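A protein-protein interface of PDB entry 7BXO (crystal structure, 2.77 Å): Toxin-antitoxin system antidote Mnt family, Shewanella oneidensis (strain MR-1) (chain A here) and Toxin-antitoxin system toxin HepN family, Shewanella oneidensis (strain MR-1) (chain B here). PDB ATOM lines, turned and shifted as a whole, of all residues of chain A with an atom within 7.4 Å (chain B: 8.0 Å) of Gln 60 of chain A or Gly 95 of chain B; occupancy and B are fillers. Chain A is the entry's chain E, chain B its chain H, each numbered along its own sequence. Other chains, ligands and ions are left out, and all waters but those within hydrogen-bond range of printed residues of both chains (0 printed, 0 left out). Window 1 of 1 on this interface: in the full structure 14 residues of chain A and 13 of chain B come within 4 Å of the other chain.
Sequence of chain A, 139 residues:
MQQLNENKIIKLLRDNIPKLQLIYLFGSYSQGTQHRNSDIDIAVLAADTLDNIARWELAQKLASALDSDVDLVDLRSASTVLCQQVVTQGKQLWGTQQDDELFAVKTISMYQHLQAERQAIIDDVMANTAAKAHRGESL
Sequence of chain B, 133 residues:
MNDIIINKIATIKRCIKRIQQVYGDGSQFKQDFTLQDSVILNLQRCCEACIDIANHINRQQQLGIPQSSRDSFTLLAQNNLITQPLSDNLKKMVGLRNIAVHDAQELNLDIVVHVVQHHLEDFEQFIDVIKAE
Along chain B the printed residues that touch a printed residue of chain A span positions 70 to 111. Among the printed residues, 13 pairs touch across the chains. Among the printed residues, Asp or Glu carboxylates within 4 Å of a Lys or Arg side-chain nitrogen of the other chain: Glu 57 of chain A with Lys 92 of chain B (3.2 Å) and Asp 69 of chain A with Arg 70 of chain B (2.7 Å).
O of Trp 56 of chain A lies close to NE2 of Gln 60 of chain A (3.5 Å). The backbone carbonyl oxygen (O) of Ala 63 of chain A sits at hydrogen-bond distance from the backbone NH (N) of Ser 68 of chain A (3.2 Å). The guanidinium group (NH1) of Arg 70 of chain B is in hydrogen-bond range of the backbone carbonyl oxygen (O) of Lys 91 of chain B, at 3.1 Å. The side-chain carboxylate (OD1) of Asp 88 of chain B is in salt-bridge range of the side-chain amino group (NZ) of Lys 91 of chain B (3.9 Å). NZ of Lys 92 of chain B sits at hydrogen-bond distance from OD1 of Asn 89 of chain B (2.8 Å).
Trp 56 of chain A touches Lys 92 of chain B. Trp 56 of chain A touches Leu 96 of chain B (CZ2 to CD2, 3.9 Å). CD1 of Trp 56 of chain A touches CD1 of Ile 99 of chain B, at 3.6 Å. Trp 56 of chain A touches Ile 111 of chain B (CG to CG2, 3.6 Å). OE1 of Gln 60 of chain A touches NH1 of Arg 70 of chain B, 3.8 Å away. Gln 60 of chain A touches Gly 95 of chain B. NH1 of Arg 70 of chain B touches CB of Ala 63 of chain A, 3.5 Å away. Lys 91 of chain B touches Ser 64 of chain A. C of Ser 68 of chain A touches NH2 of Arg 70 of chain B (3.9 Å).
The side-chain amino group of Lys 92 of chain B is in salt-bridge range of the side-chain carboxylate of Glu 57 of chain A, 3.2 Å away. The backbone carbonyl oxygen (O) of Lys 92 of chain B lies close to the side-chain amide oxygen (OE1) of Gln 60 of chain A, 3.5 Å away. The side-chain carboxylate (OD1) of Asp 69 of chain A is in salt-bridge range of the guanidinium group (NH2) of Arg 70 of chain B (2.7 Å). The side-chain amide nitrogen (ND2) of Asn 98 of chain B lies within hydrogen-bond range of the side-chain carboxylate (OD2) of Asp 69 of chain A.
Of chain B, only Arg 70 (3.8 Å), Lys 92 (3.5 Å) and Gly 95 (3.4 Å) come within 4 Å of Gln 60 of chain A. Of chain A, only Gln 60 (3.4 Å) comes within 4 Å of Gly 95 of chain B. Of the printed residues of chain A, Asn 98 of chain B touches Asp 69 (3.2 Å). Of the printed residues of chain B, Ser 68 of chain A touches Arg 70. Of the printed residues of chain A, Arg 70 of chain B touches Gln 60 (3.8 Å), Ala 63 (3.5 Å), Ser 68 (3.9 Å) and Asp 69 (2.7 Å). Ala 100 of chain B touches none of the printed residues of chain A. The nearest residue of chain B that does not touch Gln 60 of chain A is Lys 91 of chain B (4.6 Å).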
ATOM      1  N   ALA A  54     -32.789 -12.275  -8.706  1.00  0.00           N
ATOM      2  CA  ALA A  54     -32.629 -12.879 -10.034  1.00  0.00           C
ATOM      3  C   ALA A  54     -31.173 -12.762 -10.500  1.00  0.00           C
ATOM      4  O   ALA A  54     -30.627 -13.705 -11.074  1.00  0.00           O
ATOM      5  CB  ALA A  54     -33.557 -12.201 -11.032  1.00  0.00           C
ATOM      6  N   ARG A  55     -30.544 -11.616 -10.203  1.00  0.00           N
ATOM      7  CA  ARG A  55     -29.156 -11.312 -10.524  1.00  0.00           C
ATOM      8  C   ARG A  55     -28.212 -12.230  -9.730  1.00  0.00           C
ATOM      9  O   ARG A  55     -27.348 -12.872 -10.327  1.00  0.00           O
ATOM     10  CB  ARG A  55     -28.876  -9.831 -10.233  1.00  0.00           C
ATOM     11  CG  ARG A  55     -27.879  -9.201 -11.190  1.00  0.00           C
ATOM     12  CD  ARG A  55     -26.697  -8.601 -10.461  1.00  0.00           C
ATOM     13  NE  ARG A  55     -27.069  -7.440  -9.652  1.00  0.00           N
ATOM     14  CZ  ARG A  55     -27.164  -7.449  -8.326  1.00  0.00           C
ATOM     15  NH1 ARG A  55     -26.908  -8.557  -7.640  1.00  0.00           N
ATOM     16  NH2 ARG A  55     -27.521  -6.350  -7.674  1.00  0.00           N
ATOM     17  N   TRP A  56     -28.410 -12.317  -8.398  1.00  0.00           N
ATOM     18  CA  TRP A  56     -27.628 -13.166  -7.506  1.00  0.00           C
ATOM     19  C   TRP A  56     -27.770 -14.631  -7.893  1.00  0.00           C
ATOM     20  O   TRP A  56     -26.766 -15.328  -7.976  1.00  0.00           O
ATOM     21  CB  TRP A  56     -28.041 -12.960  -6.042  1.00  0.00           C
ATOM     22  CG  TRP A  56     -27.208 -13.749  -5.070  1.00  0.00           C
ATOM     23  CD1 TRP A  56     -25.988 -13.403  -4.564  1.00  0.00           C
ATOM     24  CD2 TRP A  56     -27.522 -15.035  -4.518  1.00  0.00           C
ATOM     25  NE1 TRP A  56     -25.536 -14.378  -3.704  1.00  0.00           N
ATOM     26  CE2 TRP A  56     -26.455 -15.396  -3.663  1.00  0.00           C
ATOM     27  CE3 TRP A  56     -28.605 -15.921  -4.661  1.00  0.00           C
ATOM     28  CZ2 TRP A  56     -26.442 -16.602  -2.951  1.00  0.00           C
ATOM     29  CZ3 TRP A  56     -28.589 -17.119  -3.960  1.00  0.00           C
ATOM     30  CH2 TRP A  56     -27.515 -17.451  -3.121  1.00  0.00           C
ATOM     31  N   GLU A  57     -29.004 -15.091  -8.151  1.00  0.00           N
ATOM     32  CA  GLU A  57     -29.271 -16.464  -8.573  1.00  0.00           C
ATOM     33  C   GLU A  57     -28.535 -16.774  -9.885  1.00  0.00           C
ATOM     34  O   GLU A  57     -27.935 -17.843 -10.007  1.00  0.00           O
ATOM     35  CB  GLU A  57     -30.785 -16.717  -8.691  1.00  0.00           C
ATOM     36  CG  GLU A  57     -31.494 -16.911  -7.353  1.00  0.00           C
ATOM     37  CD  GLU A  57     -31.553 -18.320  -6.784  1.00  0.00           C
ATOM     38  OE1 GLU A  57     -31.034 -19.257  -7.435  1.00  0.00           O
ATOM     39  OE2 GLU A  57     -32.129 -18.486  -5.684  1.00  0.00           O
ATOM     40  N   LEU A  58     -28.519 -15.811 -10.832  1.00  0.00           N
ATOM     41  CA  LEU A  58     -27.819 -15.948 -12.113  1.00  0.00           C
ATOM     42  C   LEU A  58     -26.307 -15.954 -11.930  1.00  0.00           C
ATOM     43  O   LEU A  58     -25.628 -16.731 -12.604  1.00  0.00           O
ATOM     44  CB  LEU A  58     -28.260 -14.870 -13.112  1.00  0.00           C
ATOM     45  CG  LEU A  58     -27.677 -14.930 -14.532  1.00  0.00           C
ATOM     46  CD1 LEU A  58     -27.830 -16.316 -15.164  1.00  0.00           C
ATOM     47  CD2 LEU A  58     -28.270 -13.855 -15.389  1.00  0.00           C
ATOM     48  N   ALA A  59     -25.787 -15.124 -10.995  1.00  0.00           N
ATOM     49  CA  ALA A  59     -24.363 -15.072 -10.642  1.00  0.00           C
ATOM     50  C   ALA A  59     -23.909 -16.452 -10.159  1.00  0.00           C
ATOM     51  O   ALA A  59     -22.832 -16.902 -10.542  1.00  0.00           O
ATOM     52  CB  ALA A  59     -24.125 -14.032  -9.561  1.00  0.00           C
ATOM     53  N   GLN A  60     -24.765 -17.146  -9.373  1.00  0.00           N
ATOM     54  CA  GLN A  60     -24.492 -18.489  -8.833  1.00  0.00           C
ATOM     55  C   GLN A  60     -24.575 -19.580  -9.897  1.00  0.00           C
ATOM     56  O   GLN A  60     -23.850 -20.573  -9.801  1.00  0.00           O
ATOM     57  CB  GLN A  60     -25.379 -18.808  -7.616  1.00  0.00           C
ATOM     58  CG  GLN A  60     -25.279 -17.787  -6.471  1.00  0.00           C
ATOM     59  CD  GLN A  60     -23.883 -17.236  -6.241  1.00  0.00           C
ATOM     60  OE1 GLN A  60     -22.962 -17.941  -5.814  1.00  0.00           O
ATOM     61  NE2 GLN A  60     -23.696 -15.963  -6.530  1.00  0.00           N
ATOM     62  N   LYS A  61     -25.442 -19.378 -10.921  1.00  0.00           N
ATOM     63  CA  LYS A  61     -25.623 -20.272 -12.073  1.00  0.00           C
ATOM     64  C   LYS A  61     -24.350 -20.220 -12.910  1.00  0.00           C
ATOM     65  O   LYS A  61     -23.866 -21.267 -13.333  1.00  0.00           O
ATOM     66  CB  LYS A  61     -26.854 -19.848 -12.907  1.00  0.00           C
ATOM     67  CG  LYS A  61     -27.280 -20.856 -13.981  1.00  0.00           C
ATOM     68  CD  LYS A  61     -28.784 -20.819 -14.286  1.00  0.00           C
ATOM     69  CE  LYS A  61     -29.654 -21.532 -13.260  1.00  0.00           C
ATOM     70  NZ  LYS A  61     -29.399 -23.002 -13.196  1.00  0.00           N
ATOM     71  N   LEU A  62     -23.790 -19.005 -13.112  1.00  0.00           N
ATOM     72  CA  LEU A  62     -22.527 -18.810 -13.827  1.00  0.00           C
ATOM     73  C   LEU A  62     -21.387 -19.414 -12.999  1.00  0.00           C
ATOM     74  O   LEU A  62     -20.591 -20.181 -13.540  1.00  0.00           O
ATOM     75  CB  LEU A  62     -22.279 -17.314 -14.112  1.00  0.00           C
ATOM     76  CG  LEU A  62     -22.647 -16.808 -15.526  1.00  0.00           C
ATOM     77  CD1 LEU A  62     -24.144 -16.686 -15.705  1.00  0.00           C
ATOM     78  CD2 LEU A  62     -22.044 -15.461 -15.787  1.00  0.00           C
ATOM     79  N   ALA A  63     -21.379 -19.142 -11.668  1.00  0.00           N
ATOM     80  CA  ALA A  63     -20.410 -19.651 -10.696  1.00  0.00           C
ATOM     81  C   ALA A  63     -20.297 -21.178 -10.684  1.00  0.00           C
ATOM     82  O   ALA A  63     -19.189 -21.692 -10.549  1.00  0.00           O
ATOM     83  CB  ALA A  63     -20.729 -19.128  -9.310  1.00  0.00           C
ATOM     84  N   SER A  64     -21.430 -21.899 -10.835  1.00  0.00           N
ATOM     85  CA  SER A  64     -21.449 -23.363 -10.901  1.00  0.00           C
ATOM     86  C   SER A  64     -20.816 -23.841 -12.226  1.00  0.00           C
ATOM     87  O   SER A  64     -19.943 -24.708 -12.214  1.00  0.00           O
ATOM     88  CB  SER A  64     -22.876 -23.885 -10.787  1.00  0.00           C
ATOM     89  OG  SER A  64     -23.132 -24.444  -9.509  1.00  0.00           O
ATOM     90  N   ALA A  65     -21.241 -23.237 -13.355  1.00  0.00           N
ATOM     91  CA  ALA A  65     -20.780 -23.540 -14.704  1.00  0.00           C
ATOM     92  C   ALA A  65     -19.311 -23.216 -14.925  1.00  0.00           C
ATOM     93  O   ALA A  65     -18.651 -23.915 -15.693  1.00  0.00           O
ATOM     94  CB  ALA A  65     -21.629 -22.796 -15.711  1.00  0.00           C
ATOM     95  N   LEU A  66     -18.799 -22.164 -14.263  1.00  0.00           N
ATOM     96  CA  LEU A  66     -17.404 -21.729 -14.392  1.00  0.00           C
ATOM     97  C   LEU A  66     -16.497 -22.213 -13.260  1.00  0.00           C
ATOM     98  O   LEU A  66     -15.287 -22.004 -13.331  1.00  0.00           O
ATOM     99  CB  LEU A  66     -17.323 -20.196 -14.532  1.00  0.00           C
ATOM    100  CG  LEU A  66     -18.026 -19.573 -15.743  1.00  0.00           C
ATOM    101  CD1 LEU A  66     -18.261 -18.114 -15.520  1.00  0.00           C
ATOM    102  CD2 LEU A  66     -17.243 -19.799 -17.035  1.00  0.00           C
ATOM    103  N   SER A  68     -16.077 -21.143 -10.123  1.00  0.00           N
ATOM    104  CA  SER A  68     -15.397 -20.005  -9.501  1.00  0.00           C
ATOM    105  C   SER A  68     -16.428 -19.015  -8.986  1.00  0.00           C
ATOM    106  O   SER A  68     -17.507 -18.941  -9.564  1.00  0.00           O
ATOM    107  CB  SER A  68     -14.487 -19.325 -10.525  1.00  0.00           C
ATOM    108  OG  SER A  68     -14.167 -17.989 -10.173  1.00  0.00           O
ATOM    109  N   ASP A  69     -16.094 -18.234  -7.930  1.00  0.00           N
ATOM    110  CA  ASP A  69     -16.971 -17.189  -7.386  1.00  0.00           C
ATOM    111  C   ASP A  69     -17.213 -16.177  -8.507  1.00  0.00           C
ATOM    112  O   ASP A  69     -16.271 -15.798  -9.199  1.00  0.00           O
ATOM    113  CB  ASP A  69     -16.320 -16.479  -6.178  1.00  0.00           C
ATOM    114  CG  ASP A  69     -16.484 -17.120  -4.808  1.00  0.00           C
ATOM    115  OD1 ASP A  69     -17.016 -18.240  -4.735  1.00  0.00           O
ATOM    116  OD2 ASP A  69     -16.071 -16.496  -3.808  1.00  0.00           O
ATOM    117  N   VAL A  70     -18.474 -15.806  -8.740  1.00  0.00           N
ATOM    118  CA  VAL A  70     -18.838 -14.882  -9.804  1.00  0.00           C
ATOM    119  C   VAL A  70     -19.569 -13.674  -9.248  1.00  0.00           C
ATOM    120  O   VAL A  70     -20.590 -13.814  -8.574  1.00  0.00           O
ATOM    121  CB  VAL A  70     -19.609 -15.591 -10.965  1.00  0.00           C
ATOM    122  CG1 VAL A  70     -20.290 -14.585 -11.898  1.00  0.00           C
ATOM    123  CG2 VAL A  70     -18.688 -16.519 -11.755  1.00  0.00           C
ATOM    124  N   ASP A  71     -19.041 -12.487  -9.552  1.00  0.00           N
ATOM    125  CA  ASP A  71     -19.632 -11.209  -9.181  1.00  0.00           C
ATOM    126  C   ASP A  71     -20.271 -10.640 -10.446  1.00  0.00           C
ATOM    127  O   ASP A  71     -19.561 -10.308 -11.400  1.00  0.00           O
ATOM    128  CB  ASP A  71     -18.553 -10.263  -8.631  1.00  0.00           C
ATOM    129  CG  ASP A  71     -18.986  -9.495  -7.398  1.00  0.00           C
ATOM    130  OD1 ASP A  71     -19.557  -8.383  -7.558  1.00  0.00           O
ATOM    131  OD2 ASP A  71     -18.751  -9.998  -6.268  1.00  0.00           O
ATOM    132  N   LEU A  72     -21.621 -10.611 -10.481  1.00  0.00           N
ATOM    133  CA  LEU A  72     -22.420 -10.089 -11.598  1.00  0.00           C
ATOM    134  C   LEU A  72     -22.952  -8.707 -11.218  1.00  0.00           C
ATOM    135  O   LEU A  72     -23.534  -8.541 -10.155  1.00  0.00           O
ATOM    136  CB  LEU A  72     -23.547 -11.073 -11.991  1.00  0.00           C
ATOM    137  CG  LEU A  72     -24.438 -10.726 -13.206  1.00  0.00           C
ATOM    138  CD1 LEU A  72     -23.634 -10.544 -14.485  1.00  0.00           C
ATOM    139  CD2 LEU A  72     -25.480 -11.795 -13.430  1.00  0.00           C
ATOM    140  N   GLN B  44     -22.371 -18.291   6.478  1.00  0.00           N
ATOM    141  CA  GLN B  44     -21.019 -18.716   6.089  1.00  0.00           C
ATOM    142  C   GLN B  44     -20.587 -19.936   6.905  1.00  0.00           C
ATOM    143  O   GLN B  44     -19.928 -20.825   6.369  1.00  0.00           O
ATOM    144  CB  GLN B  44     -20.010 -17.589   6.319  1.00  0.00           C
ATOM    145  CG  GLN B  44     -20.074 -16.455   5.300  1.00  0.00           C
ATOM    146  CD  GLN B  44     -19.194 -15.275   5.667  1.00  0.00           C
ATOM    147  OE1 GLN B  44     -18.244 -15.367   6.463  1.00  0.00           O
ATOM    148  NE2 GLN B  44     -19.490 -14.133   5.075  1.00  0.00           N
ATOM    149  N   CYS B  47     -22.387 -22.952   5.551  1.00  0.00           N
ATOM    150  CA  CYS B  47     -21.753 -23.229   4.273  1.00  0.00           C
ATOM    151  C   CYS B  47     -20.452 -23.995   4.426  1.00  0.00           C
ATOM    152  O   CYS B  47     -20.301 -25.037   3.793  1.00  0.00           O
ATOM    153  CB  CYS B  47     -21.566 -21.948   3.473  1.00  0.00           C
ATOM    154  SG  CYS B  47     -20.976 -22.225   1.788  1.00  0.00           S
ATOM    155  N   ILE B  51     -19.366 -27.802   3.446  1.00  0.00           N
ATOM    156  CA  ILE B  51     -18.156 -28.052   2.653  1.00  0.00           C
ATOM    157  C   ILE B  51     -17.257 -29.064   3.386  1.00  0.00           C
ATOM    158  O   ILE B  51     -16.823 -30.037   2.771  1.00  0.00           O
ATOM    159  CB  ILE B  51     -17.425 -26.735   2.241  1.00  0.00           C
ATOM    160  CG1 ILE B  51     -18.244 -25.951   1.191  1.00  0.00           C
ATOM    161  CG2 ILE B  51     -16.008 -27.016   1.719  1.00  0.00           C
ATOM    162  CD1 ILE B  51     -18.024 -24.431   1.179  1.00  0.00           C
ATOM    163  N   SER B  69     -14.553 -25.762  -3.604  1.00  0.00           N
ATOM    164  CA  SER B  69     -15.614 -25.877  -2.591  1.00  0.00           C
ATOM    165  C   SER B  69     -16.892 -26.432  -3.233  1.00  0.00           C
ATOM    166  O   SER B  69     -17.561 -27.273  -2.630  1.00  0.00           O
ATOM    167  CB  SER B  69     -15.910 -24.519  -1.963  1.00  0.00           C
ATOM    168  OG  SER B  69     -14.806 -23.987  -1.252  1.00  0.00           O
ATOM    169  N   ARG B  70     -17.214 -25.960  -4.465  1.00  0.00           N
ATOM    170  CA  ARG B  70     -18.366 -26.384  -5.270  1.00  0.00           C
ATOM    171  C   ARG B  70     -18.200 -27.829  -5.716  1.00  0.00           C
ATOM    172  O   ARG B  70     -19.157 -28.598  -5.651  1.00  0.00           O
ATOM    173  CB  ARG B  70     -18.547 -25.469  -6.490  1.00  0.00           C
ATOM    174  CG  ARG B  70     -19.459 -24.285  -6.212  1.00  0.00           C
ATOM    175  CD  ARG B  70     -19.427 -23.260  -7.322  1.00  0.00           C
ATOM    176  NE  ARG B  70     -18.764 -22.040  -6.877  1.00  0.00           N
ATOM    177  CZ  ARG B  70     -19.401 -20.969  -6.421  1.00  0.00           C
ATOM    178  NH1 ARG B  70     -20.727 -20.949  -6.365  1.00  0.00           N
ATOM    179  NH2 ARG B  70     -18.718 -19.909  -6.022  1.00  0.00           N
ATOM    180  N   ASP B  88     -26.822 -28.272  -6.427  1.00  0.00           N
ATOM    181  CA  ASP B  88     -26.943 -26.968  -7.073  1.00  0.00           C
ATOM    182  C   ASP B  88     -27.304 -25.876  -6.080  1.00  0.00           C
ATOM    183  O   ASP B  88     -26.799 -24.766  -6.206  1.00  0.00           O
ATOM    184  CB  ASP B  88     -27.966 -27.017  -8.225  1.00  0.00           C
ATOM    185  CG  ASP B  88     -27.609 -27.906  -9.414  1.00  0.00           C
ATOM    186  OD1 ASP B  88     -26.421 -28.309  -9.533  1.00  0.00           O
ATOM    187  OD2 ASP B  88     -28.518 -28.199 -10.227  1.00  0.00           O
ATOM    188  N   ASN B  89     -28.152 -26.190  -5.087  1.00  0.00           N
ATOM    189  CA  ASN B  89     -28.562 -25.232  -4.063  1.00  0.00           C
ATOM    190  C   ASN B  89     -27.460 -24.972  -3.055  1.00  0.00           C
ATOM    191  O   ASN B  89     -27.303 -23.830  -2.622  1.00  0.00           O
ATOM    192  CB  ASN B  89     -29.836 -25.682  -3.353  1.00  0.00           C
ATOM    193  CG  ASN B  89     -31.104 -25.347  -4.098  1.00  0.00           C
ATOM    194  OD1 ASN B  89     -31.311 -24.219  -4.559  1.00  0.00           O
ATOM    195  ND2 ASN B  89     -31.993 -26.318  -4.211  1.00  0.00           N
ATOM    196  N   LEU B  90     -26.696 -26.022  -2.678  1.00  0.00           N
ATOM    197  CA  LEU B  90     -25.597 -25.892  -1.720  1.00  0.00           C
ATOM    198  C   LEU B  90     -24.448 -25.117  -2.335  1.00  0.00           C
ATOM    199  O   LEU B  90     -23.801 -24.335  -1.641  1.00  0.00           O
ATOM    200  CB  LEU B  90     -25.137 -27.250  -1.167  1.00  0.00           C
ATOM    201  CG  LEU B  90     -26.136 -27.983  -0.244  1.00  0.00           C
ATOM    202  CD1 LEU B  90     -25.838 -29.459  -0.195  1.00  0.00           C
ATOM    203  CD2 LEU B  90     -26.175 -27.388   1.155  1.00  0.00           C
ATOM    204  N   LYS B  91     -24.245 -25.280  -3.654  1.00  0.00           N
ATOM    205  CA  LYS B  91     -23.241 -24.555  -4.426  1.00  0.00           C
ATOM    206  C   LYS B  91     -23.569 -23.065  -4.422  1.00  0.00           C
ATOM    207  O   LYS B  91     -22.654 -22.267  -4.287  1.00  0.00           O
ATOM    208  CB  LYS B  91     -23.146 -25.097  -5.860  1.00  0.00           C
ATOM    209  CG  LYS B  91     -22.554 -26.498  -5.935  1.00  0.00           C
ATOM    210  CD  LYS B  91     -22.096 -26.858  -7.330  1.00  0.00           C
ATOM    211  CE  LYS B  91     -22.988 -27.870  -7.992  1.00  0.00           C
ATOM    212  NZ  LYS B  91     -22.555 -28.149  -9.386  1.00  0.00           N
ATOM    213  N   LYS B  92     -24.876 -22.687  -4.493  1.00  0.00           N
ATOM    214  CA  LYS B  92     -25.360 -21.286  -4.468  1.00  0.00           C
ATOM    215  C   LYS B  92     -24.933 -20.547  -3.194  1.00  0.00           C
ATOM    216  O   LYS B  92     -24.781 -19.325  -3.211  1.00  0.00           O
ATOM    217  CB  LYS B  92     -26.896 -21.225  -4.560  1.00  0.00           C
ATOM    218  CG  LYS B  92     -27.494 -21.527  -5.916  1.00  0.00           C
ATOM    219  CD  LYS B  92     -29.011 -21.453  -5.846  1.00  0.00           C
ATOM    220  CE  LYS B  92     -29.672 -22.314  -6.896  1.00  0.00           C
ATOM    221  NZ  LYS B  92     -31.145 -22.392  -6.704  1.00  0.00           N
ATOM    222  N   MET B  93     -24.786 -21.299  -2.088  1.00  0.00           N
ATOM    223  CA  MET B  93     -24.402 -20.814  -0.764  1.00  0.00           C
ATOM    224  C   MET B  93     -22.912 -20.514  -0.661  1.00  0.00           C
ATOM    225  O   MET B  93     -22.520 -19.731   0.201  1.00  0.00           O
ATOM    226  CB  MET B  93     -24.811 -21.834   0.318  1.00  0.00           C
ATOM    227  CG  MET B  93     -26.286 -22.163   0.325  1.00  0.00           C
ATOM    228  SD  MET B  93     -27.309 -20.675   0.327  1.00  0.00           S
ATOM    229  CE  MET B  93     -27.862 -20.700   1.928  1.00  0.00           C
ATOM    230  N   VAL B  94     -22.080 -21.159  -1.512  1.00  0.00           N
ATOM    231  CA  VAL B  94     -20.621 -21.007  -1.553  1.00  0.00           C
ATOM    232  C   VAL B  94     -20.247 -19.550  -1.905  1.00  0.00           C
ATOM    233  O   VAL B  94     -19.245 -19.028  -1.409  1.00  0.00           O
ATOM    234  CB  VAL B  94     -19.958 -22.086  -2.471  1.00  0.00           C
ATOM    235  CG1 VAL B  94     -18.463 -21.844  -2.668  1.00  0.00           C
ATOM    236  CG2 VAL B  94     -20.210 -23.501  -1.942  1.00  0.00           C
ATOM    237  N   GLY B  95     -21.102 -18.896  -2.687  1.00  0.00           N
ATOM    238  CA  GLY B  95     -20.931 -17.509  -3.093  1.00  0.00           C
ATOM    239  C   GLY B  95     -21.254 -16.484  -2.024  1.00  0.00           C
ATOM    240  O   GLY B  95     -20.962 -15.299  -2.210  1.00  0.00           O
ATOM    241  N   LEU B  96     -21.867 -16.919  -0.908  1.00  0.00           N
ATOM    242  CA  LEU B  96     -22.234 -16.030   0.194  1.00  0.00           C
ATOM    243  C   LEU B  96     -21.031 -15.420   0.914  1.00  0.00           C
ATOM    244  O   LEU B  96     -21.070 -14.233   1.236  1.00  0.00           O
ATOM    245  CB  LEU B  96     -23.180 -16.709   1.196  1.00  0.00           C
ATOM    246  CG  LEU B  96     -24.643 -16.889   0.762  1.00  0.00           C
ATOM    247  CD1 LEU B  96     -25.394 -17.754   1.760  1.00  0.00           C
ATOM    248  CD2 LEU B  96     -25.359 -15.542   0.594  1.00  0.00           C
ATOM    249  N   ARG B  97     -19.961 -16.217   1.152  1.00  0.00           N
ATOM    250  CA  ARG B  97     -18.731 -15.758   1.818  1.00  0.00           C
ATOM    251  C   ARG B  97     -18.193 -14.467   1.184  1.00  0.00           C
ATOM    252  O   ARG B  97     -17.880 -13.520   1.900  1.00  0.00           O
ATOM    253  CB  ARG B  97     -17.662 -16.868   1.821  1.00  0.00           C
ATOM    254  CG  ARG B  97     -16.643 -16.740   2.962  1.00  0.00           C
ATOM    255  CD  ARG B  97     -15.323 -16.127   2.517  1.00  0.00           C
ATOM    256  NE  ARG B  97     -14.617 -15.498   3.634  1.00  0.00           N
ATOM    257  CZ  ARG B  97     -13.441 -14.882   3.541  1.00  0.00           C
ATOM    258  NH1 ARG B  97     -12.812 -14.805   2.373  1.00  0.00           N
ATOM    259  NH2 ARG B  97     -12.889 -14.328   4.612  1.00  0.00           N
ATOM    260  N   ASN B  98     -18.174 -14.419  -0.158  1.00  0.00           N
ATOM    261  CA  ASN B  98     -17.725 -13.296  -0.979  1.00  0.00           C
ATOM    262  C   ASN B  98     -18.650 -12.055  -0.911  1.00  0.00           C
ATOM    263  O   ASN B  98     -18.219 -10.968  -1.300  1.00  0.00           O
ATOM    264  CB  ASN B  98     -17.579 -13.773  -2.431  1.00  0.00           C
ATOM    265  CG  ASN B  98     -16.328 -13.321  -3.146  1.00  0.00           C
ATOM    266  OD1 ASN B  98     -16.389 -12.699  -4.214  1.00  0.00           O
ATOM    267  ND2 ASN B  98     -15.162 -13.649  -2.599  1.00  0.00           N
ATOM    268  N   ILE B  99     -19.906 -12.212  -0.429  1.00  0.00           N
ATOM    269  CA  ILE B  99     -20.889 -11.122  -0.358  1.00  0.00           C
ATOM    270  C   ILE B  99     -20.670 -10.209   0.859  1.00  0.00           C
ATOM    271  O   ILE B  99     -20.970  -9.017   0.771  1.00  0.00           O
ATOM    272  CB  ILE B  99     -22.369 -11.637  -0.466  1.00  0.00           C
ATOM    273  CG1 ILE B  99     -23.199 -10.742  -1.413  1.00  0.00           C
ATOM    274  CG2 ILE B  99     -23.076 -11.827   0.902  1.00  0.00           C
ATOM    275  CD1 ILE B  99     -24.387 -11.431  -2.079  1.00  0.00           C
ATOM    276  N   ALA B 100     -20.174 -10.755   1.978  1.00  0.00           N
ATOM    277  CA  ALA B 100     -19.969  -9.978   3.196  1.00  0.00           C
ATOM    278  C   ALA B 100     -18.625  -9.273   3.251  1.00  0.00           C
ATOM    279  O   ALA B 100     -18.578  -8.043   3.194  1.00  0.00           O
ATOM    280  CB  ALA B 100     -20.132 -10.869   4.407  1.00  0.00           C
ATOM    281  N   ILE B 111     -31.067 -10.257  -0.745  1.00  0.00           N
ATOM    282  CA  ILE B 111     -30.486 -11.574  -1.016  1.00  0.00           C
ATOM    283  C   ILE B 111     -30.393 -12.385   0.285  1.00  0.00           C
ATOM    284  O   ILE B 111     -30.742 -13.566   0.291  1.00  0.00           O
ATOM    285  CB  ILE B 111     -29.119 -11.412  -1.736  1.00  0.00           C
ATOM    286  CG1 ILE B 111     -29.318 -10.816  -3.148  1.00  0.00           C
ATOM    287  CG2 ILE B 111     -28.343 -12.738  -1.793  1.00  0.00           C
ATOM    288  CD1 ILE B 111     -28.164 -10.021  -3.677  1.00  0.00           C
